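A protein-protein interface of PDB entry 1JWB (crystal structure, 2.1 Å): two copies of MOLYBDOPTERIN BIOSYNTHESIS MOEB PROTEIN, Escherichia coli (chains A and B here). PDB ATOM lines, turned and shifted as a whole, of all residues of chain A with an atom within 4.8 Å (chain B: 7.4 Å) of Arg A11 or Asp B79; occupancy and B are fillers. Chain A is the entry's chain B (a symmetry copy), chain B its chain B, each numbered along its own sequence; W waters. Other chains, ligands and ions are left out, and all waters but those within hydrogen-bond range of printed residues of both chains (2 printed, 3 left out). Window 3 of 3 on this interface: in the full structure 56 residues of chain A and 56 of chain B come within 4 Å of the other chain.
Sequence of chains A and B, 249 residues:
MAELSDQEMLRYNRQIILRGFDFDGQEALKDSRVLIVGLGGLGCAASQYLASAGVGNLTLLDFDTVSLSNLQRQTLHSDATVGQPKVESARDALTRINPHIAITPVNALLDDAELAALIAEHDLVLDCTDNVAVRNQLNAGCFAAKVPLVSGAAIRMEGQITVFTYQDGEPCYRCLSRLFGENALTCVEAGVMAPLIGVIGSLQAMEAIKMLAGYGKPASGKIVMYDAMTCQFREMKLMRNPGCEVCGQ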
ATOM      1  N   GLN A   7     -10.609  14.970  16.762  1.00  0.00           N
ATOM      2  CA  GLN A   7     -11.870  15.495  17.207  1.00  0.00           C
ATOM      3  C   GLN A   7     -12.755  15.827  16.009  1.00  0.00           C
ATOM      4  O   GLN A   7     -13.953  15.676  16.043  1.00  0.00           O
ATOM      5  CB  GLN A   7     -11.644  16.699  18.103  1.00  0.00           C
ATOM      6  CG  GLN A   7     -10.975  16.323  19.393  1.00  0.00           C
ATOM      7  CD  GLN A   7      -9.432  16.067  19.266  1.00  0.00           C
ATOM      8  OE1 GLN A   7      -8.804  16.419  18.260  1.00  0.00           O
ATOM      9  NE2 GLN A   7      -8.843  15.451  20.313  1.00  0.00           N
ATOM     10  N   GLU A   8     -12.117  16.253  14.940  1.00  0.00           N
ATOM     11  CA  GLU A   8     -12.797  16.530  13.689  1.00  0.00           C
ATOM     12  C   GLU A   8     -13.373  15.263  13.084  1.00  0.00           C
ATOM     13  O   GLU A   8     -14.525  15.254  12.637  1.00  0.00           O
ATOM     14  CB  GLU A   8     -11.830  17.214  12.727  1.00  0.00           C
ATOM     15  CG  GLU A   8     -11.755  18.701  12.968  1.00  0.00           C
ATOM     16  CD  GLU A   8     -10.730  19.436  12.117  1.00  0.00           C
ATOM     17  OE1 GLU A   8      -9.719  18.823  11.679  1.00  0.00           O
ATOM     18  OE2 GLU A   8     -10.971  20.635  11.871  1.00  0.00           O
ATOM     19  N   MET A   9     -12.579  14.185  13.048  1.00  0.00           N
ATOM     20  CA  MET A   9     -13.051  12.919  12.480  1.00  0.00           C
ATOM     21  C   MET A   9     -14.274  12.385  13.185  1.00  0.00           C
ATOM     22  O   MET A   9     -15.179  11.836  12.564  1.00  0.00           O
ATOM     23  CB  MET A   9     -11.945  11.891  12.473  1.00  0.00           C
ATOM     24  CG  MET A   9     -10.888  12.209  11.391  1.00  0.00           C
ATOM     25  SD  MET A   9      -9.479  11.024  11.305  1.00  0.00           S
ATOM     26  CE  MET A   9      -8.820  11.233  12.906  1.00  0.00           C
ATOM     27  N   LEU A  10     -14.312  12.568  14.494  1.00  0.00           N
ATOM     28  CA  LEU A  10     -15.478  12.221  15.258  1.00  0.00           C
ATOM     29  C   LEU A  10     -16.646  13.132  14.925  1.00  0.00           C
ATOM     30  O   LEU A  10     -17.749  12.672  14.694  1.00  0.00           O
ATOM     31  CB  LEU A  10     -15.169  12.342  16.736  1.00  0.00           C
ATOM     32  CG  LEU A  10     -14.113  11.349  17.256  1.00  0.00           C
ATOM     33  CD1 LEU A  10     -13.576  11.809  18.624  1.00  0.00           C
ATOM     34  CD2 LEU A  10     -14.675   9.900  17.323  1.00  0.00           C
ATOM     35  N   ARG A  11     -16.419  14.428  14.931  1.00  0.00           N
ATOM     36  CA  ARG A  11     -17.489  15.361  14.632  1.00  0.00           C
ATOM     37  C   ARG A  11     -18.050  15.064  13.281  1.00  0.00           C
ATOM     38  O   ARG A  11     -19.266  15.051  13.062  1.00  0.00           O
ATOM     39  CB  ARG A  11     -16.928  16.750  14.614  1.00  0.00           C
ATOM     40  CG  ARG A  11     -17.896  17.847  14.651  1.00  0.00           C
ATOM     41  CD  ARG A  11     -17.192  19.202  14.611  1.00  0.00           C
ATOM     42  NE  ARG A  11     -18.091  20.305  14.978  1.00  0.00           N
ATOM     43  CZ  ARG A  11     -18.213  20.777  16.203  1.00  0.00           C
ATOM     44  NH1 ARG A  11     -17.497  20.235  17.181  1.00  0.00           N
ATOM     45  NH2 ARG A  11     -19.045  21.774  16.455  1.00  0.00           N
ATOM     46  N   TYR A  12     -17.181  14.759  12.350  1.00  0.00           N
ATOM     47  CA  TYR A  12     -17.695  14.625  10.983  1.00  0.00           C
ATOM     48  C   TYR A  12     -17.917  13.206  10.578  1.00  0.00           C
ATOM     49  O   TYR A  12     -18.130  12.881   9.429  1.00  0.00           O
ATOM     50  CB  TYR A  12     -16.742  15.280  10.023  1.00  0.00           C
ATOM     51  CG  TYR A  12     -16.424  16.724  10.312  1.00  0.00           C
ATOM     52  CD1 TYR A  12     -15.108  17.174  10.294  1.00  0.00           C
ATOM     53  CD2 TYR A  12     -17.414  17.656  10.524  1.00  0.00           C
ATOM     54  CE1 TYR A  12     -14.796  18.480  10.492  1.00  0.00           C
ATOM     55  CE2 TYR A  12     -17.106  19.005  10.689  1.00  0.00           C
ATOM     56  CZ  TYR A  12     -15.781  19.399  10.654  1.00  0.00           C
ATOM     57  OH  TYR A  12     -15.422  20.671  10.887  1.00  0.00           O
ATOM     58  N   ASN A  13     -17.960  12.335  11.555  1.00  0.00           N
ATOM     59  CA  ASN A  13     -18.117  10.926  11.221  1.00  0.00           C
ATOM     60  C   ASN A  13     -19.246  10.560  10.243  1.00  0.00           C
ATOM     61  O   ASN A  13     -19.081   9.729   9.342  1.00  0.00           O
ATOM     62  CB  ASN A  13     -18.286  10.171  12.532  1.00  0.00           C
ATOM     63  CG  ASN A  13     -18.450   8.683  12.324  1.00  0.00           C
ATOM     64  OD1 ASN A  13     -17.541   8.011  11.841  1.00  0.00           O
ATOM     65  ND2 ASN A  13     -19.630   8.176  12.645  1.00  0.00           N
ATOM     66  N   ARG A  96     -20.241  29.165  16.776  1.00  0.00           N
ATOM     67  CA  ARG A  96     -20.758  28.200  17.752  1.00  0.00           C
ATOM     68  C   ARG A  96     -21.228  26.887  17.091  1.00  0.00           C
ATOM     69  O   ARG A  96     -21.120  25.820  17.659  1.00  0.00           O
ATOM     70  CB  ARG A  96     -21.903  28.804  18.564  1.00  0.00           C
ATOM     71  CG  ARG A  96     -21.498  29.942  19.437  1.00  0.00           C
ATOM     72  CD  ARG A  96     -22.611  30.404  20.338  1.00  0.00           C
ATOM     73  NE  ARG A  96     -23.225  29.209  20.913  1.00  0.00           N
ATOM     74  CZ  ARG A  96     -24.519  28.920  20.844  1.00  0.00           C
ATOM     75  NH1 ARG A  96     -25.364  29.764  20.256  1.00  0.00           N
ATOM     76  NH2 ARG A  96     -24.976  27.789  21.377  1.00  0.00           N
ATOM     77  N   ILE A  97     -21.780  26.962  15.910  1.00  0.00           N
ATOM     78  CA  ILE A  97     -22.144  25.751  15.198  1.00  0.00           C
ATOM     79  C   ILE A  97     -20.916  24.941  14.922  1.00  0.00           C
ATOM     80  O   ILE A  97     -20.945  23.737  15.123  1.00  0.00           O
ATOM     81  CB  ILE A  97     -22.881  26.078  13.903  1.00  0.00           C
ATOM     82  CG1 ILE A  97     -24.275  26.626  14.227  1.00  0.00           C
ATOM     83  CG2 ILE A  97     -23.041  24.851  13.054  1.00  0.00           C
ATOM     84  CD1 ILE A  97     -24.885  27.512  13.075  1.00  0.00           C
ATOM     85  N   ASN A  98     -19.813  25.589  14.545  1.00  0.00           N
ATOM     86  CA  ASN A  98     -18.569  24.875  14.298  1.00  0.00           C
ATOM     87  C   ASN A  98     -17.372  25.791  14.546  1.00  0.00           C
ATOM     88  O   ASN A  98     -17.082  26.696  13.773  1.00  0.00           O
ATOM     89  CB  ASN A  98     -18.529  24.295  12.875  1.00  0.00           C
ATOM     90  CG  ASN A  98     -17.428  23.269  12.711  1.00  0.00           C
ATOM     91  OD1 ASN A  98     -16.494  23.261  13.489  1.00  0.00           O
ATOM     92  ND2 ASN A  98     -17.526  22.405  11.695  1.00  0.00           N
ATOM     93  N   PRO A  99     -16.702  25.553  15.678  1.00  0.00           N
ATOM     94  CA  PRO A  99     -15.551  26.367  16.080  1.00  0.00           C
ATOM     95  C   PRO A  99     -14.271  25.961  15.380  1.00  0.00           C
ATOM     96  O   PRO A  99     -13.275  26.538  15.661  1.00  0.00           O
ATOM     97  CB  PRO A  99     -15.462  26.091  17.565  1.00  0.00           C
ATOM     98  CG  PRO A  99     -15.928  24.645  17.681  1.00  0.00           C
ATOM     99  CD  PRO A  99     -16.969  24.451  16.607  1.00  0.00           C
ATOM    100  N   HIS A 100     -14.297  24.971  14.489  1.00  0.00           N
ATOM    101  CA  HIS A 100     -13.136  24.561  13.755  1.00  0.00           C
ATOM    102  C   HIS A 100     -12.995  25.318  12.476  1.00  0.00           C
ATOM    103  O   HIS A 100     -11.999  25.186  11.787  1.00  0.00           O
ATOM    104  CB  HIS A 100     -13.248  23.077  13.370  1.00  0.00           C
ATOM    105  CG  HIS A 100     -13.333  22.177  14.548  1.00  0.00           C
ATOM    106  ND1 HIS A 100     -12.305  22.099  15.476  1.00  0.00           N
ATOM    107  CD2 HIS A 100     -14.404  21.583  15.128  1.00  0.00           C
ATOM    108  CE1 HIS A 100     -12.655  21.211  16.388  1.00  0.00           C
ATOM    109  NE2 HIS A 100     -13.953  20.977  16.275  1.00  0.00           N
ATOM    110  N   VAL B  66     -27.009  14.896  23.744  1.00  0.00           N
ATOM    111  CA  VAL B  66     -26.191  15.445  22.649  1.00  0.00           C
ATOM    112  C   VAL B  66     -24.799  14.819  22.663  1.00  0.00           C
ATOM    113  O   VAL B  66     -24.139  14.784  23.703  1.00  0.00           O
ATOM    114  CB  VAL B  66     -25.962  16.978  22.838  1.00  0.00           C
ATOM    115  CG1 VAL B  66     -25.083  17.557  21.748  1.00  0.00           C
ATOM    116  CG2 VAL B  66     -27.282  17.716  22.904  1.00  0.00           C
ATOM    117  N   SER B  67     -24.345  14.392  21.501  1.00  0.00           N
ATOM    118  CA  SER B  67     -23.004  13.868  21.364  1.00  0.00           C
ATOM    119  C   SER B  67     -22.264  14.702  20.288  1.00  0.00           C
ATOM    120  O   SER B  67     -22.877  15.478  19.559  1.00  0.00           O
ATOM    121  CB  SER B  67     -23.022  12.366  21.083  1.00  0.00           C
ATOM    122  OG  SER B  67     -23.301  12.073  19.742  1.00  0.00           O
ATOM    123  N   LEU B  68     -20.952  14.547  20.225  1.00  0.00           N
ATOM    124  CA  LEU B  68     -20.096  15.366  19.380  1.00  0.00           C
ATOM    125  C   LEU B  68     -20.360  15.122  17.885  1.00  0.00           C
ATOM    126  O   LEU B  68     -20.327  16.033  17.050  1.00  0.00           O
ATOM    127  CB  LEU B  68     -18.649  15.075  19.777  1.00  0.00           C
ATOM    128  CG  LEU B  68     -17.540  15.579  18.879  1.00  0.00           C
ATOM    129  CD1 LEU B  68     -17.744  17.047  18.531  1.00  0.00           C
ATOM    130  CD2 LEU B  68     -16.177  15.357  19.500  1.00  0.00           C
ATOM    131  N   SER B  69     -20.626  13.865  17.584  1.00  0.00           N
ATOM    132  CA  SER B  69     -21.012  13.455  16.283  1.00  0.00           C
ATOM    133  C   SER B  69     -22.291  14.117  15.784  1.00  0.00           C
ATOM    134  O   SER B  69     -22.443  14.295  14.574  1.00  0.00           O
ATOM    135  CB  SER B  69     -21.239  11.973  16.244  1.00  0.00           C
ATOM    136  OG  SER B  69     -21.740  11.717  14.969  1.00  0.00           O
ATOM    137  N   ASN B  70     -23.220  14.447  16.675  1.00  0.00           N
ATOM    138  CA  ASN B  70     -24.438  15.124  16.284  1.00  0.00           C
ATOM    139  C   ASN B  70     -24.179  16.515  15.717  1.00  0.00           C
ATOM    140  O   ASN B  70     -25.005  17.084  14.995  1.00  0.00           O
ATOM    141  CB  ASN B  70     -25.304  15.406  17.499  1.00  0.00           C
ATOM    142  CG  ASN B  70     -25.725  14.195  18.233  1.00  0.00           C
ATOM    143  OD1 ASN B  70     -26.142  14.313  19.395  1.00  0.00           O
ATOM    144  ND2 ASN B  70     -25.625  13.020  17.595  1.00  0.00           N
ATOM    145  N   LEU B  71     -23.060  17.108  16.119  1.00  0.00           N
ATOM    146  CA  LEU B  71     -22.814  18.502  15.819  1.00  0.00           C
ATOM    147  C   LEU B  71     -22.507  18.742  14.363  1.00  0.00           C
ATOM    148  O   LEU B  71     -22.428  19.889  13.898  1.00  0.00           O
ATOM    149  CB  LEU B  71     -21.683  19.004  16.722  1.00  0.00           C
ATOM    150  CG  LEU B  71     -21.969  18.893  18.237  1.00  0.00           C
ATOM    151  CD1 LEU B  71     -20.815  19.465  19.030  1.00  0.00           C
ATOM    152  CD2 LEU B  71     -23.229  19.644  18.601  1.00  0.00           C
ATOM    153  N   GLN B  72     -22.295  17.668  13.638  1.00  0.00           N
ATOM    154  CA  GLN B  72     -22.060  17.777  12.227  1.00  0.00           C
ATOM    155  C   GLN B  72     -23.368  18.199  11.577  1.00  0.00           C
ATOM    156  O   GLN B  72     -23.358  18.838  10.563  1.00  0.00           O
ATOM    157  CB  GLN B  72     -21.599  16.419  11.702  1.00  0.00           C
ATOM    158  CG  GLN B  72     -21.956  16.152  10.198  1.00  0.00           C
ATOM    159  CD  GLN B  72     -23.186  15.269  10.044  1.00  0.00           C
ATOM    160  OE1 GLN B  72     -23.713  14.737  11.068  1.00  0.00           O
ATOM    161  NE2 GLN B  72     -23.636  15.067   8.793  1.00  0.00           N
ATOM    162  N   ARG B  73     -24.503  17.857  12.175  1.00  0.00           N
ATOM    163  CA  ARG B  73     -25.767  18.262  11.562  1.00  0.00           C
ATOM    164  C   ARG B  73     -26.875  18.817  12.475  1.00  0.00           C
ATOM    165  O   ARG B  73     -27.756  19.507  11.996  1.00  0.00           O
ATOM    166  CB  ARG B  73     -26.365  17.098  10.753  1.00  0.00           C
ATOM    167  CG  ARG B  73     -26.813  15.952  11.618  1.00  0.00           C
ATOM    168  CD  ARG B  73     -27.088  14.718  10.888  1.00  0.00           C
ATOM    169  NE  ARG B  73     -27.587  13.693  11.789  1.00  0.00           N
ATOM    170  CZ  ARG B  73     -26.854  12.958  12.567  1.00  0.00           C
ATOM    171  NH1 ARG B  73     -25.544  13.091  12.602  1.00  0.00           N
ATOM    172  NH2 ARG B  73     -27.443  12.094  13.349  1.00  0.00           N
ATOM    173  N   HIS B  77     -27.747  22.158  18.617  1.00  0.00           N
ATOM    174  CA  HIS B  77     -26.839  21.714  19.677  1.00  0.00           C
ATOM    175  C   HIS B  77     -25.431  22.229  19.440  1.00  0.00           C
ATOM    176  O   HIS B  77     -25.107  22.654  18.333  1.00  0.00           O
ATOM    177  CB  HIS B  77     -26.822  20.196  19.787  1.00  0.00           C
ATOM    178  CG  HIS B  77     -28.180  19.583  19.798  1.00  0.00           C
ATOM    179  ND1 HIS B  77     -29.177  20.013  20.658  1.00  0.00           N
ATOM    180  CD2 HIS B  77     -28.701  18.538  19.107  1.00  0.00           C
ATOM    181  CE1 HIS B  77     -30.285  19.387  20.322  1.00  0.00           C
ATOM    182  NE2 HIS B  77     -29.947  18.317  19.629  1.00  0.00           N
ATOM    183  N   SER B  78     -24.598  22.172  20.479  1.00  0.00           N
ATOM    184  CA  SER B  78     -23.255  22.677  20.373  1.00  0.00           C
ATOM    185  C   SER B  78     -22.293  21.929  21.263  1.00  0.00           C
ATOM    186  O   SER B  78     -22.678  21.044  22.053  1.00  0.00           O
ATOM    187  CB  SER B  78     -23.239  24.175  20.698  1.00  0.00           C
ATOM    188  OG  SER B  78     -23.573  24.425  22.059  1.00  0.00           O
ATOM    189  N   ASP B  79     -21.009  22.241  21.098  1.00  0.00           N
ATOM    190  CA  ASP B  79     -19.985  21.579  21.884  1.00  0.00           C
ATOM    191  C   ASP B  79     -20.242  21.824  23.327  1.00  0.00           C
ATOM    192  O   ASP B  79     -20.094  20.968  24.131  1.00  0.00           O
ATOM    193  CB  ASP B  79     -18.606  22.136  21.503  1.00  0.00           C
ATOM    194  CG  ASP B  79     -18.277  21.831  20.094  1.00  0.00           C
ATOM    195  OD1 ASP B  79     -18.647  22.639  19.196  1.00  0.00           O
ATOM    196  OD2 ASP B  79     -17.725  20.753  19.819  1.00  0.00           O
ATOM    197  N   ALA B  80     -20.660  23.021  23.660  1.00  0.00           N
ATOM    198  CA  ALA B  80     -20.992  23.335  25.012  1.00  0.00           C
ATOM    199  C   ALA B  80     -22.191  22.581  25.549  1.00  0.00           C
ATOM    200  O   ALA B  80     -22.350  22.520  26.765  1.00  0.00           O
ATOM    201  CB  ALA B  80     -21.203  24.789  25.136  1.00  0.00           C
ATOM    202  N   THR B  81     -23.040  22.004  24.691  1.00  0.00           N
ATOM    203  CA  THR B  81     -24.185  21.243  25.205  1.00  0.00           C
ATOM    204  C   THR B  81     -23.994  19.761  25.111  1.00  0.00           C
ATOM    205  O   THR B  81     -24.892  18.989  25.437  1.00  0.00           O
ATOM    206  CB  THR B  81     -25.547  21.622  24.537  1.00  0.00           C
ATOM    207  OG1 THR B  81     -25.582  21.291  23.129  1.00  0.00           O
ATOM    208  CG2 THR B  81     -25.774  23.109  24.662  1.00  0.00           C
ATOM    209  N   VAL B  82     -22.836  19.346  24.657  1.00  0.00           N
ATOM    210  CA  VAL B  82     -22.544  17.915  24.632  1.00  0.00           C
ATOM    211  C   VAL B  82     -22.796  17.368  26.047  1.00  0.00           C
ATOM    212  O   VAL B  82     -22.404  17.972  27.024  1.00  0.00           O
ATOM    213  CB  VAL B  82     -21.128  17.655  24.133  1.00  0.00           C
ATOM    214  CG1 VAL B  82     -20.764  16.161  24.283  1.00  0.00           C
ATOM    215  CG2 VAL B  82     -21.018  18.020  22.650  1.00  0.00           C
ATOM    216  N   GLY B  83     -23.529  16.267  26.125  1.00  0.00           N
ATOM    217  CA  GLY B  83     -23.842  15.619  27.380  1.00  0.00           C
ATOM    218  C   GLY B  83     -25.222  15.994  27.840  1.00  0.00           C
ATOM    219  O   GLY B  83     -25.793  15.305  28.660  1.00  0.00           O
HETATM  220  O   HOH W   1     -20.195  20.932  12.997  1.00  0.00           O
HETATM  221  O   HOH W   2     -19.611  24.905  19.699  1.00  0.00           O
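Among the printed residues, merely in contact across the chains: Leu A10 with Ser B69 (3.7 Å), Arg A11 with Leu B68 (3.5 Å), Arg A11 with Ser B69 (3.6 Å), Arg A11 with Leu B71 (3.8 Å), Arg A11 with Gln B72 (3.0 Å), Arg A96 with Ser B78 (3.7 Å) and Pro A99 with Asp B79 (3.6 Å).
The guanidinium group (NH1) of Arg A11 lies within salt-bridge range of the side-chain carboxylate (OD2) of Asp B79 (2.7 Å).
No position is printed for both chains.
Of the 12 printed residues of chain A, 4 touch a printed residue of chain B.
Hydrophobic or aromatic side chains of chain A that line the printed part of chain B: Pro A99.
Among the printed residues, 8 pairs touch across the chains.
Among the printed residues, Asp or Glu carboxylates within 4 Å of a Lys or Arg side-chain nitrogen of the other chain: Arg A11 with Asp B79.
N of Ser B78 sits at hydrogen-bond distance from OG1 of Thr B81.
The backbone carbonyl oxygen of Ile A97 lies within hydrogen-bond range of the guanidinium group of Arg A11 (3.0 Å).
The side-chain amide oxygen of Gln B72 is in hydrogen-bond range of the guanidinium group of Arg B73 (2.9 Å).
Water W2 bridges the side-chain carboxylate of Asp B79 (2.5 Å) and the backbone carbonyl oxygen of Arg A96 (2.7 Å).
Water W1 lies within hydrogen-bond range of O of Leu B71 (2.6 Å), NE of Arg A11 (3.0 Å) and ND2 of Asn A98 (3.3 Å).
Of chain B, only Leu B68, Ser B69, Leu B71, Gln B72 and Asp B79 come within 4 Å of Arg A11.
Printed residues of chain B within 4 Å of Pro A99: Asp B79.
Of the printed residues of chain A, Ser B69 touches Leu A10 and Arg A11.
Asp B79 touches two residues of chain A.
The nearest residue of chain B that does not touch Arg A11 is Asn B70 (5.4 Å).
The nearest residue of chain A that does not touch Asp B79 is Arg A96 (4.3 Å).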
